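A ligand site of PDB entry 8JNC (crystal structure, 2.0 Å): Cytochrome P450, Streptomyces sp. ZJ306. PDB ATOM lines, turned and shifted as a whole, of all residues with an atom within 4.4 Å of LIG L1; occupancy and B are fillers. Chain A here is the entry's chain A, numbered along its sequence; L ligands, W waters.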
ATOM      1  N   LEU A  67      -3.543  24.162  14.542  1.00  0.00           N
ATOM      2  CA  LEU A  67      -4.426  24.482  13.448  1.00  0.00           C
ATOM      3  C   LEU A  67      -5.909  24.317  13.767  1.00  0.00           C
ATOM      4  O   LEU A  67      -6.753  24.936  13.097  1.00  0.00           O
ATOM      5  CB  LEU A  67      -4.051  23.601  12.254  1.00  0.00           C
ATOM      6  CG  LEU A  67      -2.729  23.861  11.541  1.00  0.00           C
ATOM      7  CD1 LEU A  67      -2.503  22.650  10.624  1.00  0.00           C
ATOM      8  CD2 LEU A  67      -2.713  25.165  10.770  1.00  0.00           C
ATOM      9  N   LEU A  95     -10.342  35.390   4.852  1.00  0.00           N
ATOM     10  CA  LEU A  95     -10.570  34.203   5.671  1.00  0.00           C
ATOM     11  C   LEU A  95      -9.449  33.962   6.672  1.00  0.00           C
ATOM     12  O   LEU A  95      -9.706  33.443   7.766  1.00  0.00           O
ATOM     13  CB  LEU A  95     -10.743  32.976   4.788  1.00  0.00           C
ATOM     14  CG  LEU A  95     -12.069  33.027   4.007  1.00  0.00           C
ATOM     15  CD1 LEU A  95     -11.975  32.006   2.922  1.00  0.00           C
ATOM     16  CD2 LEU A  95     -13.265  32.804   4.908  1.00  0.00           C
ATOM     17  N   PHE A  96      -8.229  34.342   6.315  1.00  0.00           N
ATOM     18  CA  PHE A  96      -7.043  34.203   7.156  1.00  0.00           C
ATOM     19  C   PHE A  96      -6.957  35.273   8.257  1.00  0.00           C
ATOM     20  O   PHE A  96      -6.093  35.204   9.138  1.00  0.00           O
ATOM     21  CB  PHE A  96      -5.784  34.272   6.285  1.00  0.00           C
ATOM     22  CG  PHE A  96      -5.399  32.959   5.630  1.00  0.00           C
ATOM     23  CD1 PHE A  96      -5.062  31.852   6.385  1.00  0.00           C
ATOM     24  CD2 PHE A  96      -5.322  32.858   4.262  1.00  0.00           C
ATOM     25  CE1 PHE A  96      -4.673  30.631   5.771  1.00  0.00           C
ATOM     26  CE2 PHE A  96      -4.920  31.657   3.649  1.00  0.00           C
ATOM     27  CZ  PHE A  96      -4.599  30.551   4.409  1.00  0.00           C
ATOM     28  N   HIS A 103     -15.143  33.708  11.272  1.00  0.00           N
ATOM     29  CA  HIS A 103     -14.607  33.082  10.094  1.00  0.00           C
ATOM     30  C   HIS A 103     -15.640  32.148   9.485  1.00  0.00           C
ATOM     31  O   HIS A 103     -15.859  32.071   8.268  1.00  0.00           O
ATOM     32  CB  HIS A 103     -13.335  32.280  10.481  1.00  0.00           C
ATOM     33  CG  HIS A 103     -12.912  31.237   9.488  1.00  0.00           C
ATOM     34  ND1 HIS A 103     -13.196  29.883   9.618  1.00  0.00           N
ATOM     35  CD2 HIS A 103     -12.185  31.354   8.348  1.00  0.00           C
ATOM     36  CE1 HIS A 103     -12.622  29.217   8.637  1.00  0.00           C
ATOM     37  NE2 HIS A 103     -12.052  30.090   7.821  1.00  0.00           N
ATOM     38  N   ARG A 107     -16.832  32.221   5.601  1.00  0.00           N
ATOM     39  CA  ARG A 107     -16.524  31.101   4.721  1.00  0.00           C
ATOM     40  C   ARG A 107     -17.798  30.478   4.174  1.00  0.00           C
ATOM     41  O   ARG A 107     -17.839  30.016   3.038  1.00  0.00           O
ATOM     42  CB  ARG A 107     -15.710  30.059   5.479  1.00  0.00           C
ATOM     43  CG  ARG A 107     -15.052  29.058   4.595  1.00  0.00           C
ATOM     44  CD  ARG A 107     -14.093  28.137   5.409  1.00  0.00           C
ATOM     45  NE  ARG A 107     -13.862  26.888   4.700  1.00  0.00           N
ATOM     46  CZ  ARG A 107     -12.658  26.323   4.568  1.00  0.00           C
ATOM     47  NH1 ARG A 107     -11.564  26.921   4.967  1.00  0.00           N
ATOM     48  NH2 ARG A 107     -12.556  25.127   4.024  1.00  0.00           N
ATOM     49  N   PHE A 114     -17.302  24.584  -3.076  1.00  0.00           N
ATOM     50  CA  PHE A 114     -16.060  23.808  -2.949  1.00  0.00           C
ATOM     51  C   PHE A 114     -16.253  22.435  -2.304  1.00  0.00           C
ATOM     52  O   PHE A 114     -15.279  21.682  -2.165  1.00  0.00           O
ATOM     53  CB  PHE A 114     -15.000  24.647  -2.202  1.00  0.00           C
ATOM     54  CG  PHE A 114     -14.479  25.808  -3.051  1.00  0.00           C
ATOM     55  CD1 PHE A 114     -13.400  25.644  -3.893  1.00  0.00           C
ATOM     56  CD2 PHE A 114     -15.097  27.047  -3.002  1.00  0.00           C
ATOM     57  CE1 PHE A 114     -12.962  26.698  -4.692  1.00  0.00           C
ATOM     58  CE2 PHE A 114     -14.648  28.093  -3.783  1.00  0.00           C
ATOM     59  CZ  PHE A 114     -13.588  27.902  -4.637  1.00  0.00           C
ATOM     60  N   VAL A 159      -9.724  28.411 -12.082  1.00  0.00           N
ATOM     61  CA  VAL A 159     -10.352  29.380 -11.157  1.00  0.00           C
ATOM     62  C   VAL A 159     -10.796  30.695 -11.825  1.00  0.00           C
ATOM     63  O   VAL A 159     -11.782  31.316 -11.389  1.00  0.00           O
ATOM     64  CB  VAL A 159      -9.479  29.727  -9.931  1.00  0.00           C
ATOM     65  CG1 VAL A 159      -9.446  28.545  -9.009  1.00  0.00           C
ATOM     66  CG2 VAL A 159      -8.141  30.189 -10.337  1.00  0.00           C
ATOM     67  N   ASP A 241      -9.015  36.409  -1.688  1.00  0.00           N
ATOM     68  CA  ASP A 241      -8.494  35.153  -1.150  1.00  0.00           C
ATOM     69  C   ASP A 241      -8.423  34.098  -2.242  1.00  0.00           C
ATOM     70  O   ASP A 241      -7.410  33.408  -2.419  1.00  0.00           O
ATOM     71  CB  ASP A 241      -9.383  34.631  -0.010  1.00  0.00           C
ATOM     72  CG  ASP A 241      -9.193  35.398   1.316  1.00  0.00           C
ATOM     73  OD1 ASP A 241      -8.165  36.081   1.513  1.00  0.00           O
ATOM     74  OD2 ASP A 241     -10.137  35.310   2.147  1.00  0.00           O
ATOM     75  N   LEU A 242      -9.523  33.930  -2.985  1.00  0.00           N
ATOM     76  CA  LEU A 242      -9.583  32.851  -3.970  1.00  0.00           C
ATOM     77  C   LEU A 242      -8.673  33.130  -5.152  1.00  0.00           C
ATOM     78  O   LEU A 242      -8.150  32.188  -5.761  1.00  0.00           O
ATOM     79  CB  LEU A 242     -11.003  32.637  -4.453  1.00  0.00           C
ATOM     80  CG  LEU A 242     -12.022  32.051  -3.500  1.00  0.00           C
ATOM     81  CD1 LEU A 242     -13.397  31.984  -4.161  1.00  0.00           C
ATOM     82  CD2 LEU A 242     -11.558  30.700  -3.016  1.00  0.00           C
ATOM     83  N   ALA A 245      -4.938  32.573  -3.765  1.00  0.00           N
ATOM     84  CA  ALA A 245      -4.570  31.246  -3.335  1.00  0.00           C
ATOM     85  C   ALA A 245      -4.797  30.210  -4.409  1.00  0.00           C
ATOM     86  O   ALA A 245      -4.245  29.125  -4.331  1.00  0.00           O
ATOM     87  CB  ALA A 245      -5.376  30.858  -2.087  1.00  0.00           C
ATOM     88  N   GLY A 246      -5.669  30.500  -5.352  1.00  0.00           N
ATOM     89  CA  GLY A 246      -6.282  29.459  -6.139  1.00  0.00           C
ATOM     90  C   GLY A 246      -5.617  28.894  -7.383  1.00  0.00           C
ATOM     91  O   GLY A 246      -6.164  27.953  -7.977  1.00  0.00           O
ATOM     92  N   SER A 249      -0.752  28.086  -6.243  1.00  0.00           N
ATOM     93  CA  SER A 249      -0.589  26.879  -5.435  1.00  0.00           C
ATOM     94  C   SER A 249      -0.460  25.640  -6.307  1.00  0.00           C
ATOM     95  O   SER A 249       0.574  24.947  -6.293  1.00  0.00           O
ATOM     96  CB  SER A 249      -1.819  26.730  -4.511  1.00  0.00           C
ATOM     97  OG  SER A 249      -3.028  26.912  -5.248  1.00  0.00           O
ATOM     98  N   THR A 250      -1.505  25.340  -7.056  1.00  0.00           N
ATOM     99  CA  THR A 250      -1.540  24.151  -7.919  1.00  0.00           C
ATOM    100  C   THR A 250      -0.475  24.209  -8.985  1.00  0.00           C
ATOM    101  O   THR A 250       0.106  23.182  -9.345  1.00  0.00           O
ATOM    102  CB  THR A 250      -2.906  24.012  -8.569  1.00  0.00           C
ATOM    103  OG1 THR A 250      -3.899  24.154  -7.558  1.00  0.00           O
ATOM    104  CG2 THR A 250      -3.004  22.650  -9.233  1.00  0.00           C
ATOM    105  N   GLN A 253       2.625  22.983  -7.447  1.00  0.00           N
ATOM    106  CA  GLN A 253       2.539  21.547  -7.106  1.00  0.00           C
ATOM    107  C   GLN A 253       2.511  20.644  -8.349  1.00  0.00           C
ATOM    108  O   GLN A 253       3.051  19.518  -8.295  1.00  0.00           O
ATOM    109  CB  GLN A 253       1.310  21.263  -6.236  1.00  0.00           C
ATOM    110  CG  GLN A 253       1.501  21.674  -4.820  1.00  0.00           C
ATOM    111  CD  GLN A 253       2.511  20.813  -4.034  1.00  0.00           C
ATOM    112  OE1 GLN A 253       3.674  20.729  -4.389  1.00  0.00           O
ATOM    113  NE2 GLN A 253       2.068  20.239  -2.932  1.00  0.00           N
ATOM    114  N   MET A 286       1.411  14.991  -1.773  1.00  0.00           N
ATOM    115  CA  MET A 286       0.952  16.067  -0.896  1.00  0.00           C
ATOM    116  C   MET A 286       1.649  15.966   0.461  1.00  0.00           C
ATOM    117  O   MET A 286       2.088  16.988   1.042  1.00  0.00           O
ATOM    118  CB  MET A 286      -0.559  15.970  -0.751  1.00  0.00           C
ATOM    119  CG  MET A 286      -1.426  16.559  -1.883  1.00  0.00           C
ATOM    120  SD  MET A 286      -1.160  18.341  -2.155  1.00  0.00           S
ATOM    121  CE  MET A 286      -1.571  18.873  -0.415  1.00  0.00           C
ATOM    122  N   SER A 296       3.122  29.488   7.084  1.00  0.00           N
ATOM    123  CA  SER A 296       1.887  30.132   6.610  1.00  0.00           C
ATOM    124  C   SER A 296       1.515  31.306   7.518  1.00  0.00           C
ATOM    125  O   SER A 296       1.910  32.460   7.261  1.00  0.00           O
ATOM    126  CB  SER A 296       0.751  29.110   6.536  1.00  0.00           C
ATOM    127  OG  SER A 296       0.644  28.363   7.753  1.00  0.00           O
ATOM    128  N   PHE A 297       0.694  31.028   8.529  1.00  0.00           N
ATOM    129  CA  PHE A 297       0.296  31.984   9.527  1.00  0.00           C
ATOM    130  C   PHE A 297       0.620  31.412  10.909  1.00  0.00           C
ATOM    131  O   PHE A 297       0.281  30.268  11.189  1.00  0.00           O
ATOM    132  CB  PHE A 297      -1.190  32.313   9.456  1.00  0.00           C
ATOM    133  CG  PHE A 297      -1.561  33.192   8.295  1.00  0.00           C
ATOM    134  CD1 PHE A 297      -1.697  32.690   7.030  1.00  0.00           C
ATOM    135  CD2 PHE A 297      -1.799  34.546   8.502  1.00  0.00           C
ATOM    136  CE1 PHE A 297      -2.064  33.526   5.943  1.00  0.00           C
ATOM    137  CE2 PHE A 297      -2.142  35.379   7.450  1.00  0.00           C
ATOM    138  CZ  PHE A 297      -2.279  34.863   6.168  1.00  0.00           C
ATOM    139  N   ARG A 299      -0.136  30.975  14.871  1.00  0.00           N
ATOM    140  CA  ARG A 299      -1.275  31.116  15.775  1.00  0.00           C
ATOM    141  C   ARG A 299      -0.757  31.599  17.128  1.00  0.00           C
ATOM    142  O   ARG A 299       0.444  31.521  17.432  1.00  0.00           O
ATOM    143  CB  ARG A 299      -2.024  29.789  15.931  1.00  0.00           C
ATOM    144  CG  ARG A 299      -3.049  29.525  14.871  1.00  0.00           C
ATOM    145  CD  ARG A 299      -2.458  29.344  13.454  1.00  0.00           C
ATOM    146  NE  ARG A 299      -3.512  28.918  12.549  1.00  0.00           N
ATOM    147  CZ  ARG A 299      -3.389  28.613  11.261  1.00  0.00           C
ATOM    148  NH1 ARG A 299      -2.238  28.703  10.624  1.00  0.00           N
ATOM    149  NH2 ARG A 299      -4.487  28.238  10.574  1.00  0.00           N
ATOM    150  N   ILE A 322       3.669  22.393   8.725  1.00  0.00           N
ATOM    151  CA  ILE A 322       2.957  21.253   8.127  1.00  0.00           C
ATOM    152  C   ILE A 322       3.928  20.273   7.480  1.00  0.00           C
ATOM    153  O   ILE A 322       3.691  19.058   7.513  1.00  0.00           O
ATOM    154  CB  ILE A 322       1.883  21.710   7.123  1.00  0.00           C
ATOM    155  CG1 ILE A 322       2.489  22.554   6.020  1.00  0.00           C
ATOM    156  CG2 ILE A 322       0.730  22.492   7.841  1.00  0.00           C
ATOM    157  CD1 ILE A 322       1.488  22.828   4.860  1.00  0.00           C
ATOM    158  N   GLY A 349      -1.144  18.381   4.590  1.00  0.00           N
ATOM    159  CA  GLY A 349      -0.729  19.200   3.455  1.00  0.00           C
ATOM    160  C   GLY A 349      -1.747  20.228   3.039  1.00  0.00           C
ATOM    161  O   GLY A 349      -1.361  21.187   2.348  1.00  0.00           O
ATOM    162  N   PHE A 350      -3.034  20.025   3.407  1.00  0.00           N
ATOM    163  CA  PHE A 350      -4.101  21.000   3.186  1.00  0.00           C
ATOM    164  C   PHE A 350      -4.487  21.682   4.506  1.00  0.00           C
ATOM    165  O   PHE A 350      -5.535  22.333   4.607  1.00  0.00           O
ATOM    166  CB  PHE A 350      -5.341  20.325   2.570  1.00  0.00           C
ATOM    167  CG  PHE A 350      -5.157  19.895   1.149  1.00  0.00           C
ATOM    168  CD1 PHE A 350      -4.778  20.800   0.158  1.00  0.00           C
ATOM    169  CD2 PHE A 350      -5.330  18.593   0.797  1.00  0.00           C
ATOM    170  CE1 PHE A 350      -4.577  20.396  -1.129  1.00  0.00           C
ATOM    171  CE2 PHE A 350      -5.155  18.163  -0.526  1.00  0.00           C
ATOM    172  CZ  PHE A 350      -4.756  19.073  -1.476  1.00  0.00           C
ATOM    173  N   GLY A 351      -3.647  21.508   5.525  1.00  0.00           N
ATOM    174  CA  GLY A 351      -3.946  22.019   6.857  1.00  0.00           C
ATOM    175  C   GLY A 351      -4.954  21.185   7.630  1.00  0.00           C
ATOM    176  O   GLY A 351      -5.086  19.970   7.451  1.00  0.00           O
ATOM    177  N   PRO A 354     -10.342  24.965  11.276  1.00  0.00           N
ATOM    178  CA  PRO A 354     -11.099  26.002  10.542  1.00  0.00           C
ATOM    179  C   PRO A 354     -10.566  26.344   9.168  1.00  0.00           C
ATOM    180  O   PRO A 354     -11.345  26.420   8.190  1.00  0.00           O
ATOM    181  CB  PRO A 354     -11.009  27.186  11.516  1.00  0.00           C
ATOM    182  CG  PRO A 354     -11.052  26.596  12.868  1.00  0.00           C
ATOM    183  CD  PRO A 354     -10.350  25.216  12.721  1.00  0.00           C
ATOM    184  N   HIS A 355      -9.243  26.592   9.061  1.00  0.00           N
ATOM    185  CA  HIS A 355      -8.635  27.117   7.846  1.00  0.00           C
ATOM    186  C   HIS A 355      -8.135  26.024   6.895  1.00  0.00           C
ATOM    187  O   HIS A 355      -7.374  26.342   5.987  1.00  0.00           O
ATOM    188  CB  HIS A 355      -7.496  28.087   8.249  1.00  0.00           C
ATOM    189  CG  HIS A 355      -7.969  29.228   9.103  1.00  0.00           C
ATOM    190  ND1 HIS A 355      -8.572  30.342   8.574  1.00  0.00           N
ATOM    191  CD2 HIS A 355      -8.056  29.352  10.453  1.00  0.00           C
ATOM    192  CE1 HIS A 355      -8.963  31.134   9.560  1.00  0.00           C
ATOM    193  NE2 HIS A 355      -8.647  30.572  10.699  1.00  0.00           N
ATOM    194  N   CYS A 357      -7.776  23.876   3.820  1.00  0.00           N
ATOM    195  CA  CYS A 357      -7.878  24.407   2.471  1.00  0.00           C
ATOM    196  C   CYS A 357      -9.252  24.269   1.833  1.00  0.00           C
ATOM    197  O   CYS A 357      -9.717  23.155   1.545  1.00  0.00           O
ATOM    198  CB  CYS A 357      -6.868  23.724   1.537  1.00  0.00           C
ATOM    199  SG  CYS A 357      -6.923  24.353  -0.117  1.00  0.00           S
ATOM    200  N   ILE A 358      -9.907  25.414   1.615  1.00  0.00           N
ATOM    201  CA  ILE A 358     -11.230  25.385   1.007  1.00  0.00           C
ATOM    202  C   ILE A 358     -11.126  24.792  -0.392  1.00  0.00           C
ATOM    203  O   ILE A 358     -12.098  24.256  -0.934  1.00  0.00           O
ATOM    204  CB  ILE A 358     -11.886  26.791   0.959  1.00  0.00           C
ATOM    205  CG1 ILE A 358     -13.380  26.647   0.601  1.00  0.00           C
ATOM    206  CG2 ILE A 358     -11.197  27.670  -0.068  1.00  0.00           C
ATOM    207  CD1 ILE A 358     -14.195  27.929   0.838  1.00  0.00           C
ATOM    208  N   GLY A 359      -9.943  24.893  -1.005  1.00  0.00           N
ATOM    209  CA  GLY A 359      -9.795  24.338  -2.340  1.00  0.00           C
ATOM    210  C   GLY A 359      -9.318  22.884  -2.411  1.00  0.00           C
ATOM    211  O   GLY A 359      -8.902  22.410  -3.475  1.00  0.00           O
ATOM    212  N   LEU A 362     -10.653  20.639  -5.177  1.00  0.00           N
ATOM    213  CA  LEU A 362     -10.332  21.134  -6.513  1.00  0.00           C
ATOM    214  C   LEU A 362      -8.857  20.880  -6.840  1.00  0.00           C
ATOM    215  O   LEU A 362      -8.532  20.521  -7.968  1.00  0.00           O
ATOM    216  CB  LEU A 362     -10.634  22.637  -6.641  1.00  0.00           C
ATOM    217  CG  LEU A 362     -10.351  23.362  -7.947  1.00  0.00           C
ATOM    218  CD1 LEU A 362     -11.252  22.732  -8.967  1.00  0.00           C
ATOM    219  CD2 LEU A 362     -10.621  24.854  -7.815  1.00  0.00           C
ATOM    220  N   ALA A 363      -7.958  21.085  -5.869  1.00  0.00           N
ATOM    221  CA  ALA A 363      -6.523  20.778  -6.065  1.00  0.00           C
ATOM    222  C   ALA A 363      -6.292  19.276  -6.331  1.00  0.00           C
ATOM    223  O   ALA A 363      -5.473  18.900  -7.202  1.00  0.00           O
ATOM    224  CB  ALA A 363      -5.745  21.210  -4.817  1.00  0.00           C
ATOM    225  N   LEU A 367      -4.707  17.862  -9.742  1.00  0.00           N
ATOM    226  CA  LEU A 367      -3.488  17.088  -9.684  1.00  0.00           C
ATOM    227  C   LEU A 367      -3.725  15.679 -10.166  1.00  0.00           C
ATOM    228  O   LEU A 367      -2.881  15.108 -10.876  1.00  0.00           O
ATOM    229  CB  LEU A 367      -2.925  17.070  -8.271  1.00  0.00           C
ATOM    230  CG  LEU A 367      -2.391  18.432  -7.876  1.00  0.00           C
ATOM    231  CD1 LEU A 367      -2.427  18.607  -6.351  1.00  0.00           C
ATOM    232  CD2 LEU A 367      -0.991  18.684  -8.392  1.00  0.00           C
HETATM  233  C1  LIG L   1      -5.727  27.503   2.884  1.00  0.00           C
HETATM  234  C2  LIG L   1      -2.673  24.330   0.908  1.00  0.00           C
HETATM  235  C3  LIG L   1      -4.789  24.899  -3.400  1.00  0.00           C
HETATM  236  C4  LIG L   1      -7.617  28.294  -1.534  1.00  0.00           C
HETATM  237  C5  LIG L   1      -4.776  26.527   2.738  1.00  0.00           C
HETATM  238  C6  LIG L   1      -3.981  25.945   3.800  1.00  0.00           C
HETATM  239  C7  LIG L   1      -3.136  25.082   3.255  1.00  0.00           C
HETATM  240  C8  LIG L   1      -3.358  25.070   1.830  1.00  0.00           C
HETATM  241  C9  LIG L   1      -2.107  24.198   3.995  1.00  0.00           C
HETATM  242  C10 LIG L   1      -4.103  26.256   5.290  1.00  0.00           C
HETATM  243  C11 LIG L   1      -2.981  27.190   5.779  1.00  0.00           C
HETATM  244  C12 LIG L   1      -3.087  27.549   7.269  1.00  0.00           C
HETATM  245  O1  LIG L   1      -4.049  27.137   7.982  1.00  0.00           O
HETATM  246  O2  LIG L   1      -2.183  28.246   7.822  1.00  0.00           O
HETATM  247  C13 LIG L   1      -2.924  24.229  -0.437  1.00  0.00           C
HETATM  248  C14 LIG L   1      -2.201  23.429  -1.434  1.00  0.00           C
HETATM  249  C15 LIG L   1      -2.812  23.620  -2.610  1.00  0.00           C
HETATM  250  C16 LIG L   1      -3.918  24.509  -2.417  1.00  0.00           C
HETATM  251  C17 LIG L   1      -0.945  22.565  -1.152  1.00  0.00           C
HETATM  252  C18 LIG L   1      -2.486  23.035  -3.989  1.00  0.00           C
HETATM  253  C19 LIG L   1      -1.782  21.918  -4.088  1.00  0.00           C
HETATM  254  C20 LIG L   1      -5.805  25.780  -3.245  1.00  0.00           C
HETATM  255  C21 LIG L   1      -6.835  26.091  -4.226  1.00  0.00           C
HETATM  256  C22 LIG L   1      -7.597  27.047  -3.679  1.00  0.00           C
HETATM  257  C23 LIG L   1      -7.078  27.346  -2.368  1.00  0.00           C
HETATM  258  C24 LIG L   1      -6.966  25.383  -5.590  1.00  0.00           C
HETATM  259  C25 LIG L   1      -8.852  27.722  -4.257  1.00  0.00           C
HETATM  260  C26 LIG L   1      -9.129  27.707  -5.573  1.00  0.00           C
HETATM  261  C27 LIG L   1      -7.353  28.437  -0.200  1.00  0.00           C
HETATM  262  C28 LIG L   1      -7.997  29.372   0.724  1.00  0.00           C
HETATM  263  C29 LIG L   1      -7.438  29.136   1.998  1.00  0.00           C
HETATM  264  C30 LIG L   1      -6.475  28.067   1.858  1.00  0.00           C
HETATM  265  C31 LIG L   1      -9.078  30.435   0.313  1.00  0.00           C
HETATM  266  C32 LIG L   1      -7.775  29.863   3.342  1.00  0.00           C
HETATM  267  C33 LIG L   1      -8.990  29.112   3.898  1.00  0.00           C
HETATM  268  C34 LIG L   1      -9.458  29.653   5.210  1.00  0.00           C
HETATM  269  O3  LIG L   1     -10.635  29.383   5.538  1.00  0.00           O
HETATM  270  O4  LIG L   1      -8.714  30.334   5.927  1.00  0.00           O
HETATM  271  N1  LIG L   1      -4.350  26.004   1.536  1.00  0.00           N
HETATM  272  N2  LIG L   1      -3.948  24.863  -1.081  1.00  0.00           N
HETATM  273  N3  LIG L   1      -5.987  26.553  -2.140  1.00  0.00           N
HETATM  274  N4  LIG L   1      -6.465  27.672   0.527  1.00  0.00           N
HETATM  275 FE1  LIG L   1      -5.419  26.069  -0.250  1.00  0.00          FE
HETATM  276  C1  LG2 L   2      -2.351  38.222   3.343  1.00  0.00           C
HETATM  277  C2  LG2 L   2      -5.058  39.189   0.800  1.00  0.00           C
HETATM  278  C3  LG2 L   2      -5.836  38.306  -0.150  1.00  0.00           C
HETATM  279  C4  LG2 L   2      -4.686  36.167   0.098  1.00  0.00           C
HETATM  280  C5  LG2 L   2      -4.816  34.769   0.589  1.00  0.00           C
HETATM  281  C6  LG2 L   2      -3.956  33.764   0.563  1.00  0.00           C
HETATM  282  C7  LG2 L   2      -2.595  33.786  -0.065  1.00  0.00           C
HETATM  283  C8  LG2 L   2      -1.587  32.961   0.745  1.00  0.00           C
HETATM  284  C9  LG2 L   2      -1.999  31.484   0.814  1.00  0.00           C
HETATM  285  C10 LG2 L   2      -0.920  30.660   1.544  1.00  0.00           C
HETATM  286  C11 LG2 L   2      -2.156  39.669   3.143  1.00  0.00           C
HETATM  287  C12 LG2 L   2      -0.634  31.255   2.922  1.00  0.00           C
HETATM  288  C13 LG2 L   2      -0.301  32.717   2.875  1.00  0.00           C
HETATM  289  C14 LG2 L   2      -1.406  33.494   2.173  1.00  0.00           C
HETATM  290  C15 LG2 L   2      -0.963  34.917   2.225  1.00  0.00           C
HETATM  291  C16 LG2 L   2      -1.718  35.894   2.663  1.00  0.00           C
HETATM  292  C17 LG2 L   2      -2.140  30.777  -0.522  1.00  0.00           C
HETATM  293  C18 LG2 L   2      -2.124  29.288  -0.139  1.00  0.00           C
HETATM  294  C19 LG2 L   2      -1.459  29.254   1.253  1.00  0.00           C
HETATM  295  C20 LG2 L   2      -1.203  28.442  -1.023  1.00  0.00           C
HETATM  296  C21 LG2 L   2      -0.855  27.318  -0.049  1.00  0.00           C
HETATM  297  C22 LG2 L   2      -0.461  28.089   1.205  1.00  0.00           C
HETATM  298  C23 LG2 L   2       0.404  26.580  -0.481  1.00  0.00           C
HETATM  299  C24 LG2 L   2       0.282  25.814  -1.748  1.00  0.00           C
HETATM  300  C25 LG2 L   2      -0.443  27.289   2.499  1.00  0.00           C
HETATM  301  C26 LG2 L   2      -4.481  39.259   3.271  1.00  0.00           C
HETATM  302  C27 LG2 L   2      -3.786  37.962   3.448  1.00  0.00           C
HETATM  303  C28 LG2 L   2      -5.582  39.343   2.223  1.00  0.00           C
HETATM  304  C29 LG2 L   2      -1.432  37.294   2.874  1.00  0.00           C
HETATM  305  N1  LG2 L   2      -5.800  36.908   0.233  1.00  0.00           N
HETATM  306  N2  LG2 L   2      -3.390  40.174   3.107  1.00  0.00           N
HETATM  307  O1  LG2 L   2      -3.645  36.634  -0.359  1.00  0.00           O
HETATM  308  O2  LG2 L   2      -4.367  36.925   3.667  1.00  0.00           O
HETATM  309  O3  LG2 L   2      -0.708  30.614   3.938  1.00  0.00           O
HETATM  310  O4  LG2 L   2      -6.314  40.569   2.340  1.00  0.00           O
HETATM  311  O5  LG2 L   2      -0.195  37.664   2.662  1.00  0.00           O
HETATM  312  O6  LG2 L   2      -1.124  40.304   3.056  1.00  0.00           O
HETATM  313  O   HOH W   1      -5.499  24.932   8.200  1.00  0.00           O
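The backbone NH of Cys 357 sits at hydrogen-bond distance from the backbone carbonyl oxygen of Phe 350. The backbone NH (N) of Gly 359 sits close to the side-chain sulfur (SG) of Cys 357 (3.2 Å). A ring nitrogen (ND1) of His 355 sits close to the backbone carbonyl oxygen (O) of Leu 95, 3.4 Å away. The guanidinium group (NH1) of Arg 107 is in hydrogen-bond range of the backbone carbonyl oxygen (O) of Pro 354, at 3.3 Å. The guanidinium group (NH1) of Arg 299 is in hydrogen-bond range of the backbone carbonyl oxygen (O) of Phe 297 (3.0 Å). The side-chain hydroxyl (OG) of Ser 249 sits at hydrogen-bond distance from the backbone carbonyl oxygen (O) of Ala 245, 2.7 Å away. The side-chain carboxylate of Asp 241 is in hydrogen-bond range of the backbone NH of Leu 95.
Leu 67 touches LIG L1 (CD2 to O1, 3.7 Å). Leu 95 touches LIG L1 (CB to O4, 3.5 Å). CE2 of Phe 96 touches C32 of LIG L1 (3.4 Å). Val 159 touches LIG L1. Ala 245 touches LIG L1. CA of Gly 246 touches C26 of LIG L1 (3.4 Å). Ser 249 touches LIG L1 (OG to C3, 3.3 Å). OG1 of Thr 250 touches C24 of LIG L1 (3.8 Å). CG of Gln 253 touches C19 of LIG L1, at 3.4 Å. CE of Met 286 touches C17 of LIG L1, 3.8 Å away. Ile 322 touches LIG L1. Gly 349 touches LIG L1 (O to C9, 3.5 Å). C of Phe 350 touches C9 of LIG L1 (3.5 Å). Gly 351 touches LIG L1. CG2 of Ile 358 touches C31 of LIG L1 (3.5 Å). Gly 359 touches LIG L1. CD2 of Leu 362 touches C26 of LIG L1, at 3.9 Å. Ala 363 touches LIG L1 (CB to C18, 3.8 Å). Hydrophobic or aromatic side chains that line LIG L1: Leu 67, Leu 95, Phe 96, His 103, Val 159, Ala 245, Met 286, Ile 322, Phe 350, His 355, Ile 358, Leu 362 and Ala 363. Of the 30 residues printed, 24 come within 4 Å of LIG L1.
An iron atom (FE1) of LIG L1 is bound by the side-chain sulfur (SG) of Cys 357, at 2.3 Å. A ring nitrogen (ND1) of His 355 lies within hydrogen-bond range of an oxygen (O4) of LIG L1. NH1 of Arg 107 lies within salt-bridge range of O3 of LIG L1, at 2.7 Å. A ring nitrogen (NE2) of His 103 sits at hydrogen-bond distance from an oxygen (O3) of LIG L1 (2.8 Å). OG of Ser 296 is in hydrogen-bond range of O2 of LIG L1 (2.8 Å). An oxygen (O2) of LIG L1 lies within salt-bridge range of the guanidinium group of Arg 299 (2.8 Å). OD1 of Asp 241 lies within hydrogen-bond range of N1 of LG2 L2, 2.8 Å away.
Water W1 bridges O1 of LIG L1 (2.6 Å) and O of His 355 (3.2 Å).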
